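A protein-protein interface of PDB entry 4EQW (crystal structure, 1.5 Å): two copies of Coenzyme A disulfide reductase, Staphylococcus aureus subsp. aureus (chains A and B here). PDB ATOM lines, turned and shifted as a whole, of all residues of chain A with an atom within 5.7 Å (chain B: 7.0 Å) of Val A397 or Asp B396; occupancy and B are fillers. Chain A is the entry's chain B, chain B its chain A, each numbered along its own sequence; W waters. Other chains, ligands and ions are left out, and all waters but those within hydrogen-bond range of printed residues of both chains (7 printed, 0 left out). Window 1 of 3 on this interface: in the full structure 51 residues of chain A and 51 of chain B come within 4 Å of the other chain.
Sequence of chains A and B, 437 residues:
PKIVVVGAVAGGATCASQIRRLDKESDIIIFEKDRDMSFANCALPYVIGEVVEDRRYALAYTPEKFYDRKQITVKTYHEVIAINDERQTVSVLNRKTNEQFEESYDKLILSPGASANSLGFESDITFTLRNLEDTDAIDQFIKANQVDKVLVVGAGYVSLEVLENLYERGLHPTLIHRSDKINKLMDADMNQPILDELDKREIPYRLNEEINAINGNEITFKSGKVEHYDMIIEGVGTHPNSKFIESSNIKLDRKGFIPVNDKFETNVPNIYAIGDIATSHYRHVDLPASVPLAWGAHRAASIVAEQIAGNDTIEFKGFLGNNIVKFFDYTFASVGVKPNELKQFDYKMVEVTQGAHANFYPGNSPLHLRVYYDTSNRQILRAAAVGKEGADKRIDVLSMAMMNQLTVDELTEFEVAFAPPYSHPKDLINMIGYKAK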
ATOM      1  N   ASP A 392      33.351  17.631  -7.678  1.00  0.00           N
ATOM      2  CA  ASP A 392      33.929  18.727  -8.452  1.00  0.00           C
ATOM      3  C   ASP A 392      33.020  19.958  -8.428  1.00  0.00           C
ATOM      4  O   ASP A 392      33.492  21.092  -8.321  1.00  0.00           O
ATOM      5  CB  ASP A 392      34.257  18.304  -9.895  1.00  0.00           C
ATOM      6  CG  ASP A 392      33.065  17.710 -10.635  1.00  0.00           C
ATOM      7  OD1 ASP A 392      32.978  17.902 -11.867  1.00  0.00           O
ATOM      8  OD2 ASP A 392      32.223  17.038 -10.000  1.00  0.00           O
ATOM      9  N   LYS A 393      31.715  19.728  -8.520  1.00  0.00           N
ATOM     10  CA  LYS A 393      30.770  20.835  -8.504  1.00  0.00           C
ATOM     11  C   LYS A 393      30.818  21.580  -7.174  1.00  0.00           C
ATOM     12  O   LYS A 393      30.916  22.816  -7.152  1.00  0.00           O
ATOM     13  CB  LYS A 393      29.347  20.362  -8.805  1.00  0.00           C
ATOM     14  CG  LYS A 393      28.324  21.514  -8.780  1.00  0.00           C
ATOM     15  CD  LYS A 393      27.008  21.140  -9.469  1.00  0.00           C
ATOM     16  CE  LYS A 393      26.269  20.041  -8.718  1.00  0.00           C
ATOM     17  NZ  LYS A 393      24.951  19.739  -9.364  1.00  0.00           N
ATOM     18  N   ARG A 394      30.772  20.845  -6.065  1.00  0.00           N
ATOM     19  CA  ARG A 394      30.758  21.501  -4.760  1.00  0.00           C
ATOM     20  C   ARG A 394      32.071  22.238  -4.496  1.00  0.00           C
ATOM     21  O   ARG A 394      32.060  23.349  -3.966  1.00  0.00           O
ATOM     22  CB  ARG A 394      30.457  20.534  -3.603  1.00  0.00           C
ATOM     23  CG  ARG A 394      29.149  19.744  -3.674  1.00  0.00           C
ATOM     24  CD  ARG A 394      28.074  20.493  -4.418  1.00  0.00           C
ATOM     25  NE  ARG A 394      26.735  19.910  -4.257  1.00  0.00           N
ATOM     26  CZ  ARG A 394      26.263  18.874  -4.948  1.00  0.00           C
ATOM     27  NH1 ARG A 394      25.016  18.467  -4.746  1.00  0.00           N
ATOM     28  NH2 ARG A 394      27.010  18.240  -5.840  1.00  0.00           N
ATOM     29  N   ILE A 395      33.201  21.641  -4.877  1.00  0.00           N
ATOM     30  CA  ILE A 395      34.479  22.307  -4.620  1.00  0.00           C
ATOM     31  C   ILE A 395      34.692  23.560  -5.487  1.00  0.00           C
ATOM     32  O   ILE A 395      35.215  24.565  -5.005  1.00  0.00           O
ATOM     33  CB  ILE A 395      35.671  21.335  -4.694  1.00  0.00           C
ATOM     34  CG1 ILE A 395      35.520  20.275  -3.603  1.00  0.00           C
ATOM     35  CG2 ILE A 395      36.986  22.100  -4.500  1.00  0.00           C
ATOM     36  CD1 ILE A 395      35.402  20.869  -2.205  1.00  0.00           C
ATOM     37  N   ASP A 396      34.247  23.527  -6.741  1.00  0.00           N
ATOM     38  CA  ASP A 396      34.324  24.728  -7.577  1.00  0.00           C
ATOM     39  C   ASP A 396      33.438  25.857  -7.028  1.00  0.00           C
ATOM     40  O   ASP A 396      33.832  27.023  -7.032  1.00  0.00           O
ATOM     41  CB  ASP A 396      33.953  24.415  -9.029  1.00  0.00           C
ATOM     42  CG  ASP A 396      35.118  23.840  -9.835  1.00  0.00           C
ATOM     43  OD1 ASP A 396      36.277  23.820  -9.355  1.00  0.00           O
ATOM     44  OD2 ASP A 396      34.871  23.414 -10.978  1.00  0.00           O
ATOM     45  N   VAL A 397      32.243  25.516  -6.551  1.00  0.00           N
ATOM     46  CA  VAL A 397      31.385  26.533  -5.959  1.00  0.00           C
ATOM     47  C   VAL A 397      32.059  27.144  -4.737  1.00  0.00           C
ATOM     48  O   VAL A 397      32.044  28.364  -4.546  1.00  0.00           O
ATOM     49  CB  VAL A 397      30.003  25.967  -5.567  1.00  0.00           C
ATOM     50  CG1 VAL A 397      29.241  26.958  -4.693  1.00  0.00           C
ATOM     51  CG2 VAL A 397      29.211  25.625  -6.825  1.00  0.00           C
ATOM     52  N   LEU A 398      32.672  26.297  -3.914  1.00  0.00           N
ATOM     53  CA  LEU A 398      33.355  26.793  -2.727  1.00  0.00           C
ATOM     54  C   LEU A 398      34.618  27.599  -3.053  1.00  0.00           C
ATOM     55  O   LEU A 398      34.938  28.541  -2.339  1.00  0.00           O
ATOM     56  CB  LEU A 398      33.629  25.656  -1.748  1.00  0.00           C
ATOM     57  CG  LEU A 398      32.334  25.141  -1.109  1.00  0.00           C
ATOM     58  CD1 LEU A 398      32.560  23.822  -0.391  1.00  0.00           C
ATOM     59  CD2 LEU A 398      31.716  26.170  -0.166  1.00  0.00           C
ATOM     60  N   SER A 399      35.309  27.247  -4.134  1.00  0.00           N
ATOM     61  CA  SER A 399      36.420  28.069  -4.611  1.00  0.00           C
ATOM     62  C   SER A 399      35.942  29.495  -4.925  1.00  0.00           C
ATOM     63  O   SER A 399      36.569  30.481  -4.530  1.00  0.00           O
ATOM     64  CB  SER A 399      37.070  27.425  -5.838  1.00  0.00           C
ATOM     65  OG  SER A 399      38.147  28.218  -6.311  1.00  0.00           O
ATOM     66  N   MET A 400      34.812  29.604  -5.617  1.00  0.00           N
ATOM     67  CA  MET A 400      34.243  30.911  -5.935  1.00  0.00           C
ATOM     68  C   MET A 400      33.792  31.654  -4.672  1.00  0.00           C
ATOM     69  O   MET A 400      33.937  32.876  -4.576  1.00  0.00           O
ATOM     70  CB  MET A 400      33.093  30.753  -6.935  1.00  0.00           C
ATOM     71  CG  MET A 400      32.370  32.051  -7.268  1.00  0.00           C
ATOM     72  SD  MET A 400      33.419  33.226  -8.136  1.00  0.00           S
ATOM     73  CE  MET A 400      33.475  32.498  -9.760  1.00  0.00           C
ATOM     74  N   ALA A 401      33.249  30.925  -3.700  1.00  0.00           N
ATOM     75  CA  ALA A 401      32.886  31.533  -2.423  1.00  0.00           C
ATOM     76  C   ALA A 401      34.107  32.123  -1.723  1.00  0.00           C
ATOM     77  O   ALA A 401      34.072  33.243  -1.227  1.00  0.00           O
ATOM     78  CB  ALA A 401      32.199  30.515  -1.520  1.00  0.00           C
ATOM     79  N   MET A 402      35.189  31.361  -1.675  1.00  0.00           N
ATOM     80  CA  MET A 402      36.396  31.831  -1.005  1.00  0.00           C
ATOM     81  C   MET A 402      37.032  33.032  -1.716  1.00  0.00           C
ATOM     82  O   MET A 402      37.613  33.899  -1.073  1.00  0.00           O
ATOM     83  CB  MET A 402      37.384  30.679  -0.842  1.00  0.00           C
ATOM     84  CG  MET A 402      36.790  29.546  -0.020  1.00  0.00           C
ATOM     85  SD  MET A 402      37.650  27.974  -0.191  1.00  0.00           S
ATOM     86  CE  MET A 402      39.121  28.300   0.754  1.00  0.00           C
ATOM     87  N   PHE A 414      23.390  30.445  -0.634  1.00  0.00           N
ATOM     88  CA  PHE A 414      23.745  29.977  -1.965  1.00  0.00           C
ATOM     89  C   PHE A 414      22.527  29.379  -2.671  1.00  0.00           C
ATOM     90  O   PHE A 414      21.927  28.420  -2.195  1.00  0.00           O
ATOM     91  CB  PHE A 414      24.897  28.957  -1.882  1.00  0.00           C
ATOM     92  CG  PHE A 414      25.076  28.123  -3.131  1.00  0.00           C
ATOM     93  CD1 PHE A 414      25.413  28.715  -4.338  1.00  0.00           C
ATOM     94  CD2 PHE A 414      24.903  26.742  -3.091  1.00  0.00           C
ATOM     95  CE1 PHE A 414      25.574  27.946  -5.492  1.00  0.00           C
ATOM     96  CE2 PHE A 414      25.057  25.966  -4.237  1.00  0.00           C
ATOM     97  CZ  PHE A 414      25.401  26.576  -5.438  1.00  0.00           C
ATOM     98  N   GLU A 415      22.178  29.948  -3.818  1.00  0.00           N
ATOM     99  CA  GLU A 415      21.013  29.481  -4.558  1.00  0.00           C
ATOM    100  C   GLU A 415      21.431  28.438  -5.595  1.00  0.00           C
ATOM    101  O   GLU A 415      21.959  28.760  -6.671  1.00  0.00           O
ATOM    102  CB  GLU A 415      20.279  30.659  -5.193  1.00  0.00           C
ATOM    103  CG  GLU A 415      18.977  30.276  -5.879  1.00  0.00           C
ATOM    104  CD  GLU A 415      18.170  31.483  -6.322  1.00  0.00           C
ATOM    105  OE1 GLU A 415      17.410  31.354  -7.308  1.00  0.00           O
ATOM    106  OE2 GLU A 415      18.307  32.557  -5.691  1.00  0.00           O
ATOM    107  N   VAL A 416      21.211  27.175  -5.249  1.00  0.00           N
ATOM    108  CA  VAL A 416      21.633  26.061  -6.088  1.00  0.00           C
ATOM    109  C   VAL A 416      20.665  25.852  -7.248  1.00  0.00           C
ATOM    110  O   VAL A 416      19.491  26.237  -7.169  1.00  0.00           O
ATOM    111  CB  VAL A 416      21.743  24.762  -5.254  1.00  0.00           C
ATOM    112  CG1 VAL A 416      20.357  24.251  -4.869  1.00  0.00           C
ATOM    113  CG2 VAL A 416      22.537  23.684  -6.005  1.00  0.00           C
ATOM    114  N   ALA A 417      21.161  25.242  -8.322  1.00  0.00           N
ATOM    115  CA  ALA A 417      20.293  24.800  -9.405  1.00  0.00           C
ATOM    116  C   ALA A 417      19.740  23.433  -9.032  1.00  0.00           C
ATOM    117  O   ALA A 417      20.471  22.437  -9.043  1.00  0.00           O
ATOM    118  CB  ALA A 417      21.069  24.724 -10.714  1.00  0.00           C
ATOM    119  N   SER A 423      20.862  17.885  -7.438  1.00  0.00           N
ATOM    120  CA  SER A 423      21.123  18.398  -6.097  1.00  0.00           C
ATOM    121  C   SER A 423      19.900  18.180  -5.205  1.00  0.00           C
ATOM    122  O   SER A 423      19.124  17.260  -5.444  1.00  0.00           O
ATOM    123  CB  SER A 423      21.462  19.892  -6.175  1.00  0.00           C
ATOM    124  OG  SER A 423      20.396  20.613  -6.787  1.00  0.00           O
ATOM    125  N   ILE A 429      25.999  22.256   0.218  1.00  0.00           N
ATOM    126  CA  ILE A 429      26.581  23.547   0.543  1.00  0.00           C
ATOM    127  C   ILE A 429      25.709  24.359   1.509  1.00  0.00           C
ATOM    128  O   ILE A 429      26.217  24.953   2.458  1.00  0.00           O
ATOM    129  CB  ILE A 429      26.909  24.350  -0.733  1.00  0.00           C
ATOM    130  CG1 ILE A 429      27.992  23.617  -1.520  1.00  0.00           C
ATOM    131  CG2 ILE A 429      27.354  25.771  -0.392  1.00  0.00           C
ATOM    132  CD1 ILE A 429      28.283  24.215  -2.873  1.00  0.00           C
ATOM    133  N   ASN B 322      18.044  30.721 -10.068  1.00  0.00           N
ATOM    134  CA  ASN B 322      18.789  29.579 -10.584  1.00  0.00           C
ATOM    135  C   ASN B 322      17.814  28.442 -10.859  1.00  0.00           C
ATOM    136  O   ASN B 322      16.983  28.115 -10.016  1.00  0.00           O
ATOM    137  CB  ASN B 322      19.864  29.140  -9.587  1.00  0.00           C
ATOM    138  CG  ASN B 322      20.970  28.335 -10.239  1.00  0.00           C
ATOM    139  OD1 ASN B 322      20.885  27.967 -11.415  1.00  0.00           O
ATOM    140  ND2 ASN B 322      22.023  28.057  -9.475  1.00  0.00           N
ATOM    141  N   ILE B 324      17.075  24.651 -13.522  1.00  0.00           N
ATOM    142  CA  ILE B 324      17.711  23.608 -14.318  1.00  0.00           C
ATOM    143  C   ILE B 324      16.705  22.506 -14.641  1.00  0.00           C
ATOM    144  O   ILE B 324      15.767  22.254 -13.869  1.00  0.00           O
ATOM    145  CB  ILE B 324      18.929  23.019 -13.555  1.00  0.00           C
ATOM    146  CG1 ILE B 324      19.735  22.063 -14.431  1.00  0.00           C
ATOM    147  CG2 ILE B 324      18.474  22.311 -12.279  1.00  0.00           C
ATOM    148  CD1 ILE B 324      21.122  21.780 -13.865  1.00  0.00           C
ATOM    149  N   ALA B 333      20.482  24.823 -18.023  1.00  0.00           N
ATOM    150  CA  ALA B 333      20.531  25.568 -16.766  1.00  0.00           C
ATOM    151  C   ALA B 333      20.714  27.062 -17.006  1.00  0.00           C
ATOM    152  O   ALA B 333      21.458  27.469 -17.899  1.00  0.00           O
ATOM    153  CB  ALA B 333      21.658  25.046 -15.876  1.00  0.00           C
ATOM    154  N   VAL B 335      20.581  31.195 -14.785  1.00  0.00           N
ATOM    155  CA  VAL B 335      20.506  31.968 -13.553  1.00  0.00           C
ATOM    156  C   VAL B 335      20.510  33.458 -13.881  1.00  0.00           C
ATOM    157  O   VAL B 335      21.109  33.881 -14.871  1.00  0.00           O
ATOM    158  CB  VAL B 335      21.658  31.611 -12.587  1.00  0.00           C
ATOM    159  CG1 VAL B 335      23.028  31.885 -13.226  1.00  0.00           C
ATOM    160  CG2 VAL B 335      21.509  32.351 -11.261  1.00  0.00           C
ATOM    161  N   ALA B 391      27.106  21.474 -17.354  1.00  0.00           N
ATOM    162  CA  ALA B 391      26.297  22.690 -17.333  1.00  0.00           C
ATOM    163  C   ALA B 391      25.875  23.065 -15.916  1.00  0.00           C
ATOM    164  O   ALA B 391      25.900  24.244 -15.546  1.00  0.00           O
ATOM    165  CB  ALA B 391      25.072  22.550 -18.236  1.00  0.00           C
ATOM    166  N   ASP B 392      25.486  22.074 -15.117  1.00  0.00           N
ATOM    167  CA  ASP B 392      25.103  22.350 -13.735  1.00  0.00           C
ATOM    168  C   ASP B 392      26.270  22.944 -12.936  1.00  0.00           C
ATOM    169  O   ASP B 392      26.096  23.912 -12.195  1.00  0.00           O
ATOM    170  CB  ASP B 392      24.502  21.118 -13.036  1.00  0.00           C
ATOM    171  CG  ASP B 392      25.392  19.891 -13.115  1.00  0.00           C
ATOM    172  OD1 ASP B 392      25.449  19.146 -12.112  1.00  0.00           O
ATOM    173  OD2 ASP B 392      26.039  19.671 -14.163  1.00  0.00           O
ATOM    174  N   LYS B 393      27.461  22.382 -13.107  1.00  0.00           N
ATOM    175  CA  LYS B 393      28.636  22.919 -12.419  1.00  0.00           C
ATOM    176  C   LYS B 393      28.918  24.395 -12.766  1.00  0.00           C
ATOM    177  O   LYS B 393      29.153  25.216 -11.869  1.00  0.00           O
ATOM    178  CB  LYS B 393      29.862  22.040 -12.686  1.00  0.00           C
ATOM    179  CG  LYS B 393      31.147  22.582 -12.052  1.00  0.00           C
ATOM    180  CD  LYS B 393      32.260  21.527 -11.997  1.00  0.00           C
ATOM    181  CE  LYS B 393      32.774  21.173 -13.388  1.00  0.00           C
ATOM    182  NZ  LYS B 393      33.904  20.190 -13.327  1.00  0.00           N
ATOM    183  N   ARG B 394      28.860  24.748 -14.044  1.00  0.00           N
ATOM    184  CA  ARG B 394      29.201  26.112 -14.441  1.00  0.00           C
ATOM    185  C   ARG B 394      28.154  27.096 -13.920  1.00  0.00           C
ATOM    186  O   ARG B 394      28.485  28.188 -13.461  1.00  0.00           O
ATOM    187  CB  ARG B 394      29.336  26.261 -15.970  1.00  0.00           C
ATOM    188  CG  ARG B 394      30.402  25.380 -16.661  1.00  0.00           C
ATOM    189  CD  ARG B 394      31.601  25.127 -15.763  1.00  0.00           C
ATOM    190  NE  ARG B 394      32.770  24.528 -16.429  1.00  0.00           N
ATOM    191  CZ  ARG B 394      32.897  23.243 -16.761  1.00  0.00           C
ATOM    192  NH1 ARG B 394      34.027  22.804 -17.318  1.00  0.00           N
ATOM    193  NH2 ARG B 394      31.910  22.385 -16.553  1.00  0.00           N
ATOM    194  N   ILE B 395      26.885  26.713 -13.992  1.00  0.00           N
ATOM    195  CA  ILE B 395      25.830  27.627 -13.577  1.00  0.00           C
ATOM    196  C   ILE B 395      25.799  27.794 -12.052  1.00  0.00           C
ATOM    197  O   ILE B 395      25.534  28.885 -11.557  1.00  0.00           O
ATOM    198  CB  ILE B 395      24.456  27.228 -14.174  1.00  0.00           C
ATOM    199  CG1 ILE B 395      24.493  27.405 -15.697  1.00  0.00           C
ATOM    200  CG2 ILE B 395      23.338  28.089 -13.598  1.00  0.00           C
ATOM    201  CD1 ILE B 395      24.857  28.821 -16.142  1.00  0.00           C
ATOM    202  N   ASP B 396      26.112  26.740 -11.303  1.00  0.00           N
ATOM    203  CA  ASP B 396      26.211  26.901  -9.850  1.00  0.00           C
ATOM    204  C   ASP B 396      27.375  27.818  -9.471  1.00  0.00           C
ATOM    205  O   ASP B 396      27.265  28.631  -8.554  1.00  0.00           O
ATOM    206  CB  ASP B 396      26.346  25.558  -9.132  1.00  0.00           C
ATOM    207  CG  ASP B 396      24.996  24.916  -8.825  1.00  0.00           C
ATOM    208  OD1 ASP B 396      23.934  25.563  -9.038  1.00  0.00           O
ATOM    209  OD2 ASP B 396      25.003  23.761  -8.350  1.00  0.00           O
ATOM    210  N   VAL B 397      28.499  27.691 -10.173  1.00  0.00           N
ATOM    211  CA  VAL B 397      29.619  28.584  -9.907  1.00  0.00           C
ATOM    212  C   VAL B 397      29.223  30.041 -10.181  1.00  0.00           C
ATOM    213  O   VAL B 397      29.562  30.936  -9.410  1.00  0.00           O
ATOM    214  CB  VAL B 397      30.888  28.195 -10.716  1.00  0.00           C
ATOM    215  CG1 VAL B 397      31.947  29.301 -10.654  1.00  0.00           C
ATOM    216  CG2 VAL B 397      31.476  26.903 -10.198  1.00  0.00           C
ATOM    217  N   LEU B 398      28.485  30.274 -11.263  1.00  0.00           N
ATOM    218  CA  LEU B 398      28.112  31.636 -11.615  1.00  0.00           C
ATOM    219  C   LEU B 398      27.030  32.180 -10.680  1.00  0.00           C
ATOM    220  O   LEU B 398      26.985  33.376 -10.420  1.00  0.00           O
ATOM    221  CB  LEU B 398      27.702  31.725 -13.089  1.00  0.00           C
ATOM    222  CG  LEU B 398      28.886  31.534 -14.046  1.00  0.00           C
ATOM    223  CD1 LEU B 398      28.407  31.444 -15.483  1.00  0.00           C
ATOM    224  CD2 LEU B 398      29.911  32.661 -13.895  1.00  0.00           C
ATOM    225  N   SER B 399      26.179  31.303 -10.153  1.00  0.00           N
ATOM    226  CA  SER B 399      25.232  31.727  -9.131  1.00  0.00           C
ATOM    227  C   SER B 399      25.998  32.278  -7.918  1.00  0.00           C
ATOM    228  O   SER B 399      25.671  33.338  -7.391  1.00  0.00           O
ATOM    229  CB  SER B 399      24.333  30.565  -8.711  1.00  0.00           C
ATOM    230  OG  SER B 399      23.470  30.968  -7.662  1.00  0.00           O
ATOM    231  N   MET B 400      27.041  31.565  -7.498  1.00  0.00           N
ATOM    232  CA  MET B 400      27.845  32.010  -6.366  1.00  0.00           C
ATOM    233  C   MET B 400      28.556  33.324  -6.706  1.00  0.00           C
ATOM    234  O   MET B 400      28.695  34.203  -5.855  1.00  0.00           O
ATOM    235  CB  MET B 400      28.851  30.925  -5.967  1.00  0.00           C
ATOM    236  CG  MET B 400      29.821  31.319  -4.852  1.00  0.00           C
ATOM    237  SD  MET B 400      29.012  31.720  -3.286  1.00  0.00           S
ATOM    238  CE  MET B 400      28.432  30.106  -2.787  1.00  0.00           C
ATOM    239  N   ALA B 401      28.994  33.463  -7.956  1.00  0.00           N
ATOM    240  CA  ALA B 401      29.628  34.709  -8.385  1.00  0.00           C
ATOM    241  C   ALA B 401      28.643  35.878  -8.311  1.00  0.00           C
ATOM    242  O   ALA B 401      28.973  36.951  -7.805  1.00  0.00           O
ATOM    243  CB  ALA B 401      30.214  34.570  -9.799  1.00  0.00           C
ATOM    244  N   PHE B 414      38.862  33.060 -11.468  1.00  0.00           N
ATOM    245  CA  PHE B 414      38.271  31.858 -10.899  1.00  0.00           C
ATOM    246  C   PHE B 414      39.259  30.698 -10.989  1.00  0.00           C
ATOM    247  O   PHE B 414      39.768  30.390 -12.065  1.00  0.00           O
ATOM    248  CB  PHE B 414      36.963  31.518 -11.622  1.00  0.00           C
ATOM    249  CG  PHE B 414      36.452  30.139 -11.322  1.00  0.00           C
ATOM    250  CD1 PHE B 414      36.096  29.781 -10.031  1.00  0.00           C
ATOM    251  CD2 PHE B 414      36.328  29.203 -12.341  1.00  0.00           C
ATOM    252  CE1 PHE B 414      35.620  28.506  -9.758  1.00  0.00           C
ATOM    253  CE2 PHE B 414      35.852  27.927 -12.074  1.00  0.00           C
ATOM    254  CZ  PHE B 414      35.512  27.579 -10.783  1.00  0.00           C
ATOM    255  N   ILE B 429      34.591  29.014 -17.744  1.00  0.00           N
ATOM    256  CA  ILE B 429      34.316  30.207 -16.949  1.00  0.00           C
ATOM    257  C   ILE B 429      35.432  31.254 -17.090  1.00  0.00           C
ATOM    258  O   ILE B 429      35.163  32.445 -17.268  1.00  0.00           O
ATOM    259  CB  ILE B 429      34.079  29.843 -15.475  1.00  0.00           C
ATOM    260  CG1 ILE B 429      32.725  29.147 -15.333  1.00  0.00           C
ATOM    261  CG2 ILE B 429      34.107  31.076 -14.607  1.00  0.00           C
ATOM    262  CD1 ILE B 429      32.438  28.627 -13.953  1.00  0.00           C
HETATM  263  O   HOH W   1      15.725  29.138  -7.385  1.00  0.00           O
HETATM  264  O   HOH W   2      26.096  22.476  -6.110  1.00  0.00           O
HETATM  265  O   HOH W   3      36.021  21.292 -11.940  1.00  0.00           O
HETATM  266  O   HOH W   4      33.813  24.636 -13.281  1.00  0.00           O
HETATM  267  O   HOH W   5      23.250  21.918  -9.214  1.00  0.00           O
HETATM  268  O   HOH W   6      17.038  25.953  -8.343  1.00  0.00           O
HETATM  269  O   HOH W   7      23.904  31.887  -4.983  1.00  0.00           O
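Of the printed residues of chain B, Asp A392 touches Lys B393 (2.9 Å). Of the printed residues of chain B, Asp A396 touches Lys B393 (3.4 Å), Val B397 (3.7 Å) and Phe B414 (3.6 Å). Of chain B, only Asp B396 (3.7 Å), Val B397 (3.98 Å) and Met B400 (3.7 Å) come within 4 Å of Val A397. Ser A399 touches none of the printed residues of chain B. Printed residues of chain B within 4 Å of Met A400: Val B397 (3.7 Å), Met B400 (3.6 Å), Ala B401 (3.7 Å) and Phe B414 (3.8 Å). Of the printed residues of chain B, Ala A401 touches Met B400. Printed residues of chain A within 4 Å of Lys B393: Asp A392 (2.9 Å), Lys A393 (3.8 Å) and Asp A396 (3.4 Å). Asp B396 touches five residues of chain A. The nearest residue of chain B that does not touch Val A397 is Lys B393 (5.1 Å). The nearest residue of chain A that does not touch Asp B396 is Glu A415 (4.4 Å). The nearest printed residue of chain A that does not touch Met B400 is Ile A429 (5.1 Å).
Lys A393 touches its own counterpart, Lys B393. Asp A396 touches Phe B414, and with the chains exchanged Phe A414 touches Asp B396. Val B397 touches its own counterpart, Val A397. Met A400 touches Phe B414, and with the chains exchanged Phe A414 touches Met B400. 12 positions are printed for both chains.
O of Glu A415 sits at hydrogen-bond distance from ND2 of Asn B322 (2.9 Å). The backbone NH (N) of Ala A417 sits close to the side-chain amide nitrogen (ND2) of Asn B322 (3.2 Å). The side-chain amino group of Lys A393 is in salt-bridge range of the side-chain carboxylate of Asp B392, at 2.9 Å. OD1 of Asp A392 is in salt-bridge range of NZ of Lys B393, 2.9 Å away. OD1 of Asp B396 is in hydrogen-bond range of N of Ala A417, at 2.9 Å. The side-chain hydroxyl of Ser B399 is in hydrogen-bond range of the backbone carbonyl oxygen of Glu A415 (2.9 Å).
Water W3 bridges OD2 of Asp A396 and NZ of Lys B393. Water W5 lies within hydrogen-bond range of OD2 of Asp B396 (2.7 Å), NZ of Lys A393 (2.8 Å) and O of Ala A417 (2.8 Å). Water W6 lies within hydrogen-bond range of the backbone carbonyl oxygen of Val A416 (2.7 Å) and the backbone carbonyl oxygen of Asn B322 (2.7 Å). Water W2 lies within hydrogen-bond range of OD2 of Asp B396 (2.8 Å) and NE of Arg A394 (3.2 Å). Water W4 bridges the side-chain carboxylate of Asp A396 (2.8 Å) and the guanidinium group of Arg B394 (3.3 Å). Water W7 lies within hydrogen-bond range of the backbone NH of Glu A415 and the side-chain hydroxyl of Ser B399.
Along chain A the printed residues that touch a printed residue of chain B span positions 392 to 417. Among the printed residues, Asp or Glu carboxylates within 4 Å of a Lys or Arg side-chain nitrogen of the other chain: Asp A392 with Lys B393 and Lys A393 with Asp B392.
ND2 of Asn B322 lies within hydrogen-bond range of OD1 of Asp B396, 3.2 Å away. The backbone carbonyl oxygen of Ala A417 lies within hydrogen-bond range of the side-chain hydroxyl of Ser A423 (2.9 Å).
Asp A396 touches Lys B393 (OD2 to CD, 3.4 Å). Val B397 touches Asp A396 (CG2 to CB, 3.7 Å). Asp A396 touches Phe B414 (O to CE1, 3.6 Å). CG2 of Val A397 touches CB of Asp B396 (3.7 Å). CG1 of Val B397 touches CE of Met A400, at 3.7 Å. Met B400 touches Met A400 (CG to CG, 3.6 Å). Ala B401 touches Met A400 (N to CG, 3.7 Å). Met A400 touches Phe B414. CD1 of Phe A414 touches CE of Met B400, at 3.7 Å. C of Val A416 touches ND2 of Asn B322 (3.4 Å).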
